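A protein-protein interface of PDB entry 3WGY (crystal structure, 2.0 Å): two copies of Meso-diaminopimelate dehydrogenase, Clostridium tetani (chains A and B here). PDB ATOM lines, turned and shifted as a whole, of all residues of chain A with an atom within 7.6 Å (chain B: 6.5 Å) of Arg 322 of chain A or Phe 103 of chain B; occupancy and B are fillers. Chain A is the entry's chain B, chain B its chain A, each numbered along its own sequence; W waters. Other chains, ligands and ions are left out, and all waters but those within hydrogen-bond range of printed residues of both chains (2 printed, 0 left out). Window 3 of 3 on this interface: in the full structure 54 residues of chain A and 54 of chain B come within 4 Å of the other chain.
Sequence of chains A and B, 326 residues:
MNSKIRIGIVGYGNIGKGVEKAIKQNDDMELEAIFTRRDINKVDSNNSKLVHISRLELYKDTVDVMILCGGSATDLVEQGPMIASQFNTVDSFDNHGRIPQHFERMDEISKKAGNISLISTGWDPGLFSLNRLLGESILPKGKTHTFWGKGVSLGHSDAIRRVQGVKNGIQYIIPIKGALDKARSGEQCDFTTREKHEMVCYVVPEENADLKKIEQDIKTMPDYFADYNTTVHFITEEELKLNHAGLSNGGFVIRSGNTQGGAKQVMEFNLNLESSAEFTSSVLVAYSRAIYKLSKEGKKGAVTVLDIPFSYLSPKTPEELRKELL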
ATOM      1  N   THR A 317     -10.765  18.832 -29.270  1.00  0.00           N
ATOM      2  CA  THR A 317     -11.962  18.677 -28.460  1.00  0.00           C
ATOM      3  C   THR A 317     -12.219  17.192 -28.248  1.00  0.00           C
ATOM      4  O   THR A 317     -11.721  16.354 -29.011  1.00  0.00           O
ATOM      5  CB  THR A 317     -13.188  19.243 -29.167  1.00  0.00           C
ATOM      6  OG1 THR A 317     -13.438  18.468 -30.347  1.00  0.00           O
ATOM      7  CG2 THR A 317     -12.968  20.706 -29.543  1.00  0.00           C
ATOM      8  N   PRO A 318     -13.002  16.849 -27.211  1.00  0.00           N
ATOM      9  CA  PRO A 318     -13.338  15.460 -26.888  1.00  0.00           C
ATOM     10  C   PRO A 318     -13.923  14.725 -28.089  1.00  0.00           C
ATOM     11  O   PRO A 318     -13.571  13.577 -28.348  1.00  0.00           O
ATOM     12  CB  PRO A 318     -14.344  15.613 -25.757  1.00  0.00           C
ATOM     13  CG  PRO A 318     -13.798  16.796 -25.029  1.00  0.00           C
ATOM     14  CD  PRO A 318     -13.504  17.754 -26.159  1.00  0.00           C
ATOM     15  N   GLU A 319     -14.809  15.394 -28.825  1.00  0.00           N
ATOM     16  CA  GLU A 319     -15.428  14.800 -30.005  1.00  0.00           C
ATOM     17  C   GLU A 319     -14.405  14.447 -31.067  1.00  0.00           C
ATOM     18  O   GLU A 319     -14.476  13.375 -31.669  1.00  0.00           O
ATOM     19  CB  GLU A 319     -16.448  15.752 -30.633  1.00  0.00           C
ATOM     20  CG  GLU A 319     -17.805  15.769 -29.978  1.00  0.00           C
ATOM     21  CD  GLU A 319     -18.804  16.600 -30.775  1.00  0.00           C
ATOM     22  OE1 GLU A 319     -18.668  17.845 -30.804  1.00  0.00           O
ATOM     23  OE2 GLU A 319     -19.712  16.000 -31.390  1.00  0.00           O
ATOM     24  N   GLU A 320     -13.470  15.361 -31.310  1.00  0.00           N
ATOM     25  CA  GLU A 320     -12.420  15.172 -32.312  1.00  0.00           C
ATOM     26  C   GLU A 320     -11.523  13.986 -31.980  1.00  0.00           C
ATOM     27  O   GLU A 320     -11.104  13.244 -32.870  1.00  0.00           O
ATOM     28  CB  GLU A 320     -11.564  16.434 -32.421  1.00  0.00           C
ATOM     29  CG  GLU A 320     -12.240  17.591 -33.144  1.00  0.00           C
ATOM     30  CD  GLU A 320     -11.412  18.864 -33.095  1.00  0.00           C
ATOM     31  OE1 GLU A 320     -11.579  19.718 -33.992  1.00  0.00           O
ATOM     32  OE2 GLU A 320     -10.599  19.018 -32.154  1.00  0.00           O
ATOM     33  N   LEU A 321     -11.222  13.824 -30.697  1.00  0.00           N
ATOM     34  CA  LEU A 321     -10.385  12.724 -30.250  1.00  0.00           C
ATOM     35  C   LEU A 321     -11.078  11.379 -30.469  1.00  0.00           C
ATOM     36  O   LEU A 321     -10.476  10.454 -31.014  1.00  0.00           O
ATOM     37  CB  LEU A 321     -10.032  12.899 -28.773  1.00  0.00           C
ATOM     38  CG  LEU A 321      -9.150  14.109 -28.445  1.00  0.00           C
ATOM     39  CD1 LEU A 321      -8.774  14.076 -26.969  1.00  0.00           C
ATOM     40  CD2 LEU A 321      -7.896  14.071 -29.305  1.00  0.00           C
ATOM     41  N   ARG A 322     -12.342  11.282 -30.059  1.00  0.00           N
ATOM     42  CA  ARG A 322     -13.111  10.048 -30.209  1.00  0.00           C
ATOM     43  C   ARG A 322     -13.323   9.651 -31.665  1.00  0.00           C
ATOM     44  O   ARG A 322     -13.443   8.470 -31.974  1.00  0.00           O
ATOM     45  CB  ARG A 322     -14.470  10.162 -29.508  1.00  0.00           C
ATOM     46  CG  ARG A 322     -14.392  10.244 -27.982  1.00  0.00           C
ATOM     47  CD  ARG A 322     -15.775  10.117 -27.343  1.00  0.00           C
ATOM     48  NE  ARG A 322     -16.632  11.277 -27.591  1.00  0.00           N
ATOM     49  CZ  ARG A 322     -16.649  12.379 -26.843  1.00  0.00           C
ATOM     50  NH1 ARG A 322     -17.465  13.379 -27.159  1.00  0.00           N
ATOM     51  NH2 ARG A 322     -15.867  12.479 -25.770  1.00  0.00           N
ATOM     52  N   LYS A 323     -13.362  10.628 -32.563  1.00  0.00           N
ATOM     53  CA  LYS A 323     -13.550  10.326 -33.978  1.00  0.00           C
ATOM     54  C   LYS A 323     -12.262   9.949 -34.709  1.00  0.00           C
ATOM     55  O   LYS A 323     -12.263   9.048 -35.546  1.00  0.00           O
ATOM     56  CB  LYS A 323     -14.189  11.513 -34.702  1.00  0.00           C
ATOM     57  CG  LYS A 323     -14.247  11.317 -36.217  1.00  0.00           C
ATOM     58  CD  LYS A 323     -15.185  12.294 -36.911  1.00  0.00           C
ATOM     59  CE  LYS A 323     -14.641  13.711 -36.895  1.00  0.00           C
ATOM     60  NZ  LYS A 323     -15.443  14.610 -37.777  1.00  0.00           N
ATOM     61  N   GLU A 324     -11.169  10.633 -34.386  1.00  0.00           N
ATOM     62  CA  GLU A 324      -9.890  10.400 -35.059  1.00  0.00           C
ATOM     63  C   GLU A 324      -8.975   9.352 -34.450  1.00  0.00           C
ATOM     64  O   GLU A 324      -8.363   8.578 -35.182  1.00  0.00           O
ATOM     65  CB  GLU A 324      -9.077  11.701 -35.145  1.00  0.00           C
ATOM     66  CG  GLU A 324      -9.836  12.913 -35.641  1.00  0.00           C
ATOM     67  CD  GLU A 324      -9.054  14.208 -35.465  1.00  0.00           C
ATOM     68  OE1 GLU A 324      -9.647  15.286 -35.655  1.00  0.00           O
ATOM     69  OE2 GLU A 324      -7.847  14.156 -35.142  1.00  0.00           O
ATOM     70  N   LEU A 325      -8.883   9.328 -33.122  1.00  0.00           N
ATOM     71  CA  LEU A 325      -7.960   8.429 -32.421  1.00  0.00           C
ATOM     72  C   LEU A 325      -8.444   7.225 -31.627  1.00  0.00           C
ATOM     73  O   LEU A 325      -7.671   6.291 -31.408  1.00  0.00           O
ATOM     74  CB  LEU A 325      -7.077   9.249 -31.472  1.00  0.00           C
ATOM     75  CG  LEU A 325      -5.959  10.106 -32.051  1.00  0.00           C
ATOM     76  CD1 LEU A 325      -5.132  10.712 -30.906  1.00  0.00           C
ATOM     77  CD2 LEU A 325      -5.084   9.244 -32.944  1.00  0.00           C
ATOM     78  N   LEU A 326      -9.688   7.243 -31.171  1.00  0.00           N
ATOM     79  CA  LEU A 326     -10.181   6.138 -30.363  1.00  0.00           C
ATOM     80  C   LEU A 326     -10.338   4.849 -31.152  1.00  0.00           C
ATOM     81  O   LEU A 326      -9.562   3.902 -30.870  1.00  0.00           O
ATOM     82  CB  LEU A 326     -11.510   6.519 -29.706  1.00  0.00           C
ATOM     83  CG  LEU A 326     -12.060   5.519 -28.689  1.00  0.00           C
ATOM     84  CD1 LEU A 326     -11.006   5.256 -27.602  1.00  0.00           C
ATOM     85  CD2 LEU A 326     -13.346   6.070 -28.070  1.00  0.00           C
ATOM     86  OXT LEU A 326     -11.220   4.807 -32.037  1.00  0.00           O
ATOM     87  N   HIS B  96     -14.659   1.274 -34.898  1.00  0.00           N
ATOM     88  CA  HIS B  96     -14.169   2.646 -34.839  1.00  0.00           C
ATOM     89  C   HIS B  96     -15.072   3.667 -35.535  1.00  0.00           C
ATOM     90  O   HIS B  96     -15.376   4.719 -34.977  1.00  0.00           O
ATOM     91  CB  HIS B  96     -12.759   2.712 -35.431  1.00  0.00           C
ATOM     92  CG  HIS B  96     -11.727   1.965 -34.634  1.00  0.00           C
ATOM     93  ND1 HIS B  96     -11.228   2.437 -33.434  1.00  0.00           N
ATOM     94  CD2 HIS B  96     -11.100   0.787 -34.868  1.00  0.00           C
ATOM     95  CE1 HIS B  96     -10.334   1.583 -32.970  1.00  0.00           C
ATOM     96  NE2 HIS B  96     -10.241   0.575 -33.818  1.00  0.00           N
ATOM     97  N   ARG B  98     -18.169   3.703 -35.930  1.00  0.00           N
ATOM     98  CA  ARG B  98     -19.441   3.936 -35.255  1.00  0.00           C
ATOM     99  C   ARG B  98     -19.336   4.343 -33.789  1.00  0.00           C
ATOM    100  O   ARG B  98     -20.349   4.485 -33.101  1.00  0.00           O
ATOM    101  CB  ARG B  98     -20.305   2.684 -35.389  1.00  0.00           C
ATOM    102  CG  ARG B  98     -20.503   2.256 -36.838  1.00  0.00           C
ATOM    103  CD  ARG B  98     -21.540   3.121 -37.532  1.00  0.00           C
ATOM    104  NE  ARG B  98     -22.897   2.724 -37.165  1.00  0.00           N
ATOM    105  CZ  ARG B  98     -23.446   1.558 -37.494  1.00  0.00           C
ATOM    106  NH1 ARG B  98     -22.755   0.672 -38.203  1.00  0.00           N
ATOM    107  NH2 ARG B  98     -24.687   1.271 -37.114  1.00  0.00           N
ATOM    108  N   ILE B  99     -18.111   4.532 -33.308  1.00  0.00           N
ATOM    109  CA  ILE B  99     -17.903   4.919 -31.918  1.00  0.00           C
ATOM    110  C   ILE B  99     -18.648   6.200 -31.560  1.00  0.00           C
ATOM    111  O   ILE B  99     -19.313   6.274 -30.527  1.00  0.00           O
ATOM    112  CB  ILE B  99     -16.400   5.088 -31.609  1.00  0.00           C
ATOM    113  CG1 ILE B  99     -15.749   3.714 -31.441  1.00  0.00           C
ATOM    114  CG2 ILE B  99     -16.212   5.904 -30.341  1.00  0.00           C
ATOM    115  CD1 ILE B  99     -14.250   3.778 -31.156  1.00  0.00           C
ATOM    116  N   PRO B 100     -18.544   7.232 -32.409  1.00  0.00           N
ATOM    117  CA  PRO B 100     -19.240   8.488 -32.118  1.00  0.00           C
ATOM    118  C   PRO B 100     -20.728   8.259 -31.835  1.00  0.00           C
ATOM    119  O   PRO B 100     -21.276   8.812 -30.883  1.00  0.00           O
ATOM    120  CB  PRO B 100     -19.004   9.308 -33.383  1.00  0.00           C
ATOM    121  CG  PRO B 100     -17.650   8.857 -33.806  1.00  0.00           C
ATOM    122  CD  PRO B 100     -17.742   7.357 -33.637  1.00  0.00           C
ATOM    123  N   GLN B 101     -21.376   7.435 -32.655  1.00  0.00           N
ATOM    124  CA  GLN B 101     -22.795   7.142 -32.467  1.00  0.00           C
ATOM    125  C   GLN B 101     -23.026   6.367 -31.177  1.00  0.00           C
ATOM    126  O   GLN B 101     -23.930   6.690 -30.401  1.00  0.00           O
ATOM    127  CB  GLN B 101     -23.354   6.334 -33.643  1.00  0.00           C
ATOM    128  CG  GLN B 101     -23.223   7.019 -34.993  1.00  0.00           C
ATOM    129  CD  GLN B 101     -21.855   6.814 -35.629  1.00  0.00           C
ATOM    130  OE1 GLN B 101     -20.819   7.012 -34.991  1.00  0.00           O
ATOM    131  NE2 GLN B 101     -21.848   6.417 -36.903  1.00  0.00           N
ATOM    132  N   HIS B 102     -22.214   5.336 -30.951  1.00  0.00           N
ATOM    133  CA  HIS B 102     -22.358   4.537 -29.741  1.00  0.00           C
ATOM    134  C   HIS B 102     -22.198   5.446 -28.522  1.00  0.00           C
ATOM    135  O   HIS B 102     -22.974   5.359 -27.571  1.00  0.00           O
ATOM    136  CB  HIS B 102     -21.314   3.416 -29.723  1.00  0.00           C
ATOM    137  CG  HIS B 102     -21.437   2.492 -28.546  1.00  0.00           C
ATOM    138  ND1 HIS B 102     -22.620   1.865 -28.210  1.00  0.00           N
ATOM    139  CD2 HIS B 102     -20.516   2.064 -27.650  1.00  0.00           C
ATOM    140  CE1 HIS B 102     -22.421   1.089 -27.160  1.00  0.00           C
ATOM    141  NE2 HIS B 102     -21.153   1.193 -26.800  1.00  0.00           N
ATOM    142  N   PHE B 103     -21.204   6.331 -28.558  1.00  0.00           N
ATOM    143  CA  PHE B 103     -20.977   7.246 -27.443  1.00  0.00           C
ATOM    144  C   PHE B 103     -22.201   8.113 -27.150  1.00  0.00           C
ATOM    145  O   PHE B 103     -22.634   8.214 -25.997  1.00  0.00           O
ATOM    146  CB  PHE B 103     -19.762   8.146 -27.713  1.00  0.00           C
ATOM    147  CG  PHE B 103     -19.432   9.080 -26.568  1.00  0.00           C
ATOM    148  CD1 PHE B 103     -20.011  10.347 -26.489  1.00  0.00           C
ATOM    149  CD2 PHE B 103     -18.575   8.676 -25.547  1.00  0.00           C
ATOM    150  CE1 PHE B 103     -19.741  11.193 -25.411  1.00  0.00           C
ATOM    151  CE2 PHE B 103     -18.301   9.515 -24.469  1.00  0.00           C
ATOM    152  CZ  PHE B 103     -18.886  10.773 -24.401  1.00  0.00           C
ATOM    153  N   GLU B 104     -22.754   8.737 -28.189  1.00  0.00           N
ATOM    154  CA  GLU B 104     -23.925   9.599 -28.029  1.00  0.00           C
ATOM    155  C   GLU B 104     -25.091   8.842 -27.406  1.00  0.00           C
ATOM    156  O   GLU B 104     -25.684   9.290 -26.418  1.00  0.00           O
ATOM    157  CB  GLU B 104     -24.367  10.174 -29.380  1.00  0.00           C
ATOM    158  CG  GLU B 104     -25.592  11.083 -29.270  1.00  0.00           C
ATOM    159  CD  GLU B 104     -26.092  11.577 -30.616  1.00  0.00           C
ATOM    160  OE1 GLU B 104     -26.584  10.751 -31.410  1.00  0.00           O
ATOM    161  OE2 GLU B 104     -25.988  12.797 -30.879  1.00  0.00           O
ATOM    162  N   ARG B 105     -25.411   7.690 -27.984  1.00  0.00           N
ATOM    163  CA  ARG B 105     -26.508   6.873 -27.490  1.00  0.00           C
ATOM    164  C   ARG B 105     -26.305   6.430 -26.039  1.00  0.00           C
ATOM    165  O   ARG B 105     -27.208   6.577 -25.208  1.00  0.00           O
ATOM    166  CB  ARG B 105     -26.690   5.651 -28.394  1.00  0.00           C
ATOM    167  CG  ARG B 105     -28.147   5.271 -28.629  1.00  0.00           C
ATOM    168  CD  ARG B 105     -28.271   4.147 -29.642  1.00  0.00           C
ATOM    169  NE  ARG B 105     -27.339   3.066 -29.338  1.00  0.00           N
ATOM    170  CZ  ARG B 105     -26.118   2.959 -29.856  1.00  0.00           C
ATOM    171  NH1 ARG B 105     -25.676   3.864 -30.724  1.00  0.00           N
ATOM    172  NH2 ARG B 105     -25.326   1.959 -29.480  1.00  0.00           N
ATOM    173  N   MET B 106     -25.126   5.890 -25.725  1.00  0.00           N
ATOM    174  CA  MET B 106     -24.862   5.446 -24.355  1.00  0.00           C
ATOM    175  C   MET B 106     -24.859   6.630 -23.397  1.00  0.00           C
ATOM    176  O   MET B 106     -25.296   6.511 -22.248  1.00  0.00           O
ATOM    177  CB  MET B 106     -23.510   4.724 -24.254  1.00  0.00           C
ATOM    178  CG  MET B 106     -23.451   3.395 -24.983  1.00  0.00           C
ATOM    179  SD  MET B 106     -24.621   2.203 -24.341  1.00  0.00           S
ATOM    180  CE  MET B 106     -23.665   1.549 -22.971  1.00  0.00           C
ATOM    181  N   ASP B 107     -24.349   7.763 -23.869  1.00  0.00           N
ATOM    182  CA  ASP B 107     -24.283   8.966 -23.048  1.00  0.00           C
ATOM    183  C   ASP B 107     -25.701   9.407 -22.687  1.00  0.00           C
ATOM    184  O   ASP B 107     -26.022   9.606 -21.516  1.00  0.00           O
ATOM    185  CB  ASP B 107     -23.540  10.086 -23.802  1.00  0.00           C
ATOM    186  CG  ASP B 107     -23.282  11.320 -22.935  1.00  0.00           C
ATOM    187  OD1 ASP B 107     -22.869  11.164 -21.767  1.00  0.00           O
ATOM    188  OD2 ASP B 107     -23.481  12.454 -23.429  1.00  0.00           O
ATOM    189  N   GLU B 108     -26.554   9.534 -23.696  1.00  0.00           N
ATOM    190  CA  GLU B 108     -27.926   9.954 -23.459  1.00  0.00           C
ATOM    191  C   GLU B 108     -28.588   9.044 -22.431  1.00  0.00           C
ATOM    192  O   GLU B 108     -29.172   9.510 -21.456  1.00  0.00           O
ATOM    193  CB  GLU B 108     -28.726   9.931 -24.765  1.00  0.00           C
ATOM    194  CG  GLU B 108     -28.179  10.853 -25.854  1.00  0.00           C
ATOM    195  CD  GLU B 108     -29.160  11.055 -27.001  1.00  0.00           C
ATOM    196  OE1 GLU B 108     -28.794  11.730 -27.988  1.00  0.00           O
ATOM    197  OE2 GLU B 108     -30.298  10.543 -26.914  1.00  0.00           O
ATOM    198  N   SER B 117     -21.203   5.084 -18.204  1.00  0.00           N
ATOM    199  CA  SER B 117     -20.918   4.057 -19.205  1.00  0.00           C
ATOM    200  C   SER B 117     -19.594   4.249 -19.924  1.00  0.00           C
ATOM    201  O   SER B 117     -19.432   5.190 -20.703  1.00  0.00           O
ATOM    202  CB  SER B 117     -22.030   4.003 -20.266  1.00  0.00           C
ATOM    203  OG  SER B 117     -23.211   3.408 -19.764  1.00  0.00           O
ATOM    204  N   ILE B 119     -17.297   3.236 -22.767  1.00  0.00           N
ATOM    205  CA  ILE B 119     -17.404   2.528 -24.035  1.00  0.00           C
ATOM    206  C   ILE B 119     -16.044   2.347 -24.690  1.00  0.00           C
ATOM    207  O   ILE B 119     -15.089   3.060 -24.396  1.00  0.00           O
ATOM    208  CB  ILE B 119     -18.273   3.290 -25.066  1.00  0.00           C
ATOM    209  CG1 ILE B 119     -17.553   4.569 -25.491  1.00  0.00           C
ATOM    210  CG2 ILE B 119     -19.639   3.597 -24.473  1.00  0.00           C
ATOM    211  CD1 ILE B 119     -18.058   5.193 -26.778  1.00  0.00           C
ATOM    212  N   GLY B 301     -22.931   9.686 -17.382  1.00  0.00           N
ATOM    213  CA  GLY B 301     -22.779   9.853 -18.815  1.00  0.00           C
ATOM    214  C   GLY B 301     -21.747   8.882 -19.362  1.00  0.00           C
ATOM    215  O   GLY B 301     -21.220   8.050 -18.632  1.00  0.00           O
ATOM    216  N   ALA B 302     -21.446   8.982 -20.648  1.00  0.00           N
ATOM    217  CA  ALA B 302     -20.473   8.081 -21.251  1.00  0.00           C
ATOM    218  C   ALA B 302     -19.060   8.645 -21.173  1.00  0.00           C
ATOM    219  O   ALA B 302     -18.860   9.862 -21.223  1.00  0.00           O
ATOM    220  CB  ALA B 302     -20.844   7.808 -22.710  1.00  0.00           C
ATOM    221  N   VAL B 303     -18.090   7.748 -21.026  1.00  0.00           N
ATOM    222  CA  VAL B 303     -16.680   8.113 -20.982  1.00  0.00           C
ATOM    223  C   VAL B 303     -15.900   7.090 -21.798  1.00  0.00           C
ATOM    224  O   VAL B 303     -16.417   6.019 -22.141  1.00  0.00           O
ATOM    225  CB  VAL B 303     -16.103   8.115 -19.539  1.00  0.00           C
ATOM    226  CG1 VAL B 303     -16.766   9.207 -18.712  1.00  0.00           C
ATOM    227  CG2 VAL B 303     -16.325   6.761 -18.881  1.00  0.00           C
ATOM    228  N   THR B 304     -14.665   7.446 -22.132  1.00  0.00           N
ATOM    229  CA  THR B 304     -13.779   6.566 -22.883  1.00  0.00           C
ATOM    230  C   THR B 304     -12.482   6.539 -22.097  1.00  0.00           C
ATOM    231  O   THR B 304     -12.307   7.332 -21.161  1.00  0.00           O
ATOM    232  CB  THR B 304     -13.471   7.100 -24.295  1.00  0.00           C
ATOM    233  OG1 THR B 304     -12.639   8.257 -24.199  1.00  0.00           O
ATOM    234  CG2 THR B 304     -14.752   7.452 -25.027  1.00  0.00           C
ATOM    235  N   LEU B 306      -9.875   7.726 -22.724  1.00  0.00           N
ATOM    236  CA  LEU B 306      -9.219   9.020 -22.806  1.00  0.00           C
ATOM    237  C   LEU B 306      -9.535   9.942 -21.626  1.00  0.00           C
ATOM    238  O   LEU B 306      -8.740  10.818 -21.291  1.00  0.00           O
ATOM    239  CB  LEU B 306      -9.604   9.720 -24.121  1.00  0.00           C
ATOM    240  CG  LEU B 306      -9.476   8.912 -25.421  1.00  0.00           C
ATOM    241  CD1 LEU B 306      -9.869   9.801 -26.590  1.00  0.00           C
ATOM    242  CD2 LEU B 306      -8.039   8.377 -25.588  1.00  0.00           C
ATOM    243  N   ASP B 307     -10.685   9.738 -20.996  1.00  0.00           N
ATOM    244  CA  ASP B 307     -11.116  10.577 -19.871  1.00  0.00           C
ATOM    245  C   ASP B 307     -10.724  10.064 -18.488  1.00  0.00           C
ATOM    246  O   ASP B 307     -10.925  10.764 -17.494  1.00  0.00           O
ATOM    247  CB  ASP B 307     -12.641  10.732 -19.884  1.00  0.00           C
ATOM    248  CG  ASP B 307     -13.181  11.122 -21.237  1.00  0.00           C
ATOM    249  OD1 ASP B 307     -12.741  12.152 -21.775  1.00  0.00           O
ATOM    250  OD2 ASP B 307     -14.050  10.395 -21.765  1.00  0.00           O
HETATM  251  O   HOH W   1     -14.722   7.394 -35.816  1.00  0.00           O
HETATM  252  O   HOH W   2     -13.736  10.725 -24.524  1.00  0.00           O
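ND1 of His 96 of chain B lies within hydrogen-bond range of OXT of Leu 326 of chain A, 2.8 Å away.
OG1 of Thr 304 of chain B lies close to N of Leu 306 of chain B (3.2 Å).
N of Thr 304 of chain B lies within hydrogen-bond range of OD2 of Asp 307 of chain B (3.0 Å).
The backbone NH (N) of Leu 326 of chain A sits at hydrogen-bond distance from the backbone carbonyl oxygen (O) of Leu 321 of chain A (3.3 Å).
Among the printed residues, pairs that only touch across the chains: Leu 326 of chain A with Ile 99 of chain B, Arg 322 of chain A with Phe 103 of chain B, Leu 326 of chain A with Thr 304 of chain B, Arg 322 of chain A with Thr 304 of chain B and Leu 321 of chain A with Leu 306 of chain B.
Of the printed residues of chain B, Leu 321 of chain A touches Leu 306 (3.8 Å).
Arg 322 of chain A touches just these residues of chain B: Phe 103 (3.6 Å) and Thr 304 (3.7 Å).
Of the printed residues of chain B, Leu 326 of chain A touches His 96, Ile 99 and Thr 304.
Printed residues of chain A within 4 Å of His 96 of chain B: Leu 326 (2.8 Å).
Phe 103 of chain B touches one residue of chain A.
Of the printed residues of chain A, Thr 304 of chain B touches Arg 322 and Leu 326.
The nearest residue of chain B that does not touch Arg 322 of chain A is Ile 99 of chain B (4.1 Å).
The nearest printed residue of chain B that does not touch Leu 321 of chain A is Asp 307 of chain B (6.8 Å).
Printed residues of chain A that touch a printed residue of chain B: Leu 321, Arg 322 and Leu 326.
Hydrophobic or aromatic side chains of chain A within 4 Å of the printed part of chain B: Leu 321 and Leu 326.
Of the 20 printed residues of chain B, 5 touch a printed residue of chain A.
Among the printed residues, no Asp or Glu carboxylate lies within 4 Å of a Lys or Arg side-chain nitrogen of the other chain.
No position is printed for both chains.
Of the 6 pairs that touch across the chains among the printed residues, none has its exchanged pair printed and touching as well.
Water W2 lies within hydrogen-bond range of the side-chain hydroxyl of Thr 304 of chain B (2.7 Å), the side-chain carboxylate of Asp 307 of chain B (2.8 Å) and the guanidinium group of Arg 322 of chain A (3.0 Å).
Water W1 lies within hydrogen-bond range of O of His 96 of chain B (2.9 Å) and O of Lys 323 of chain A (3.0 Å).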
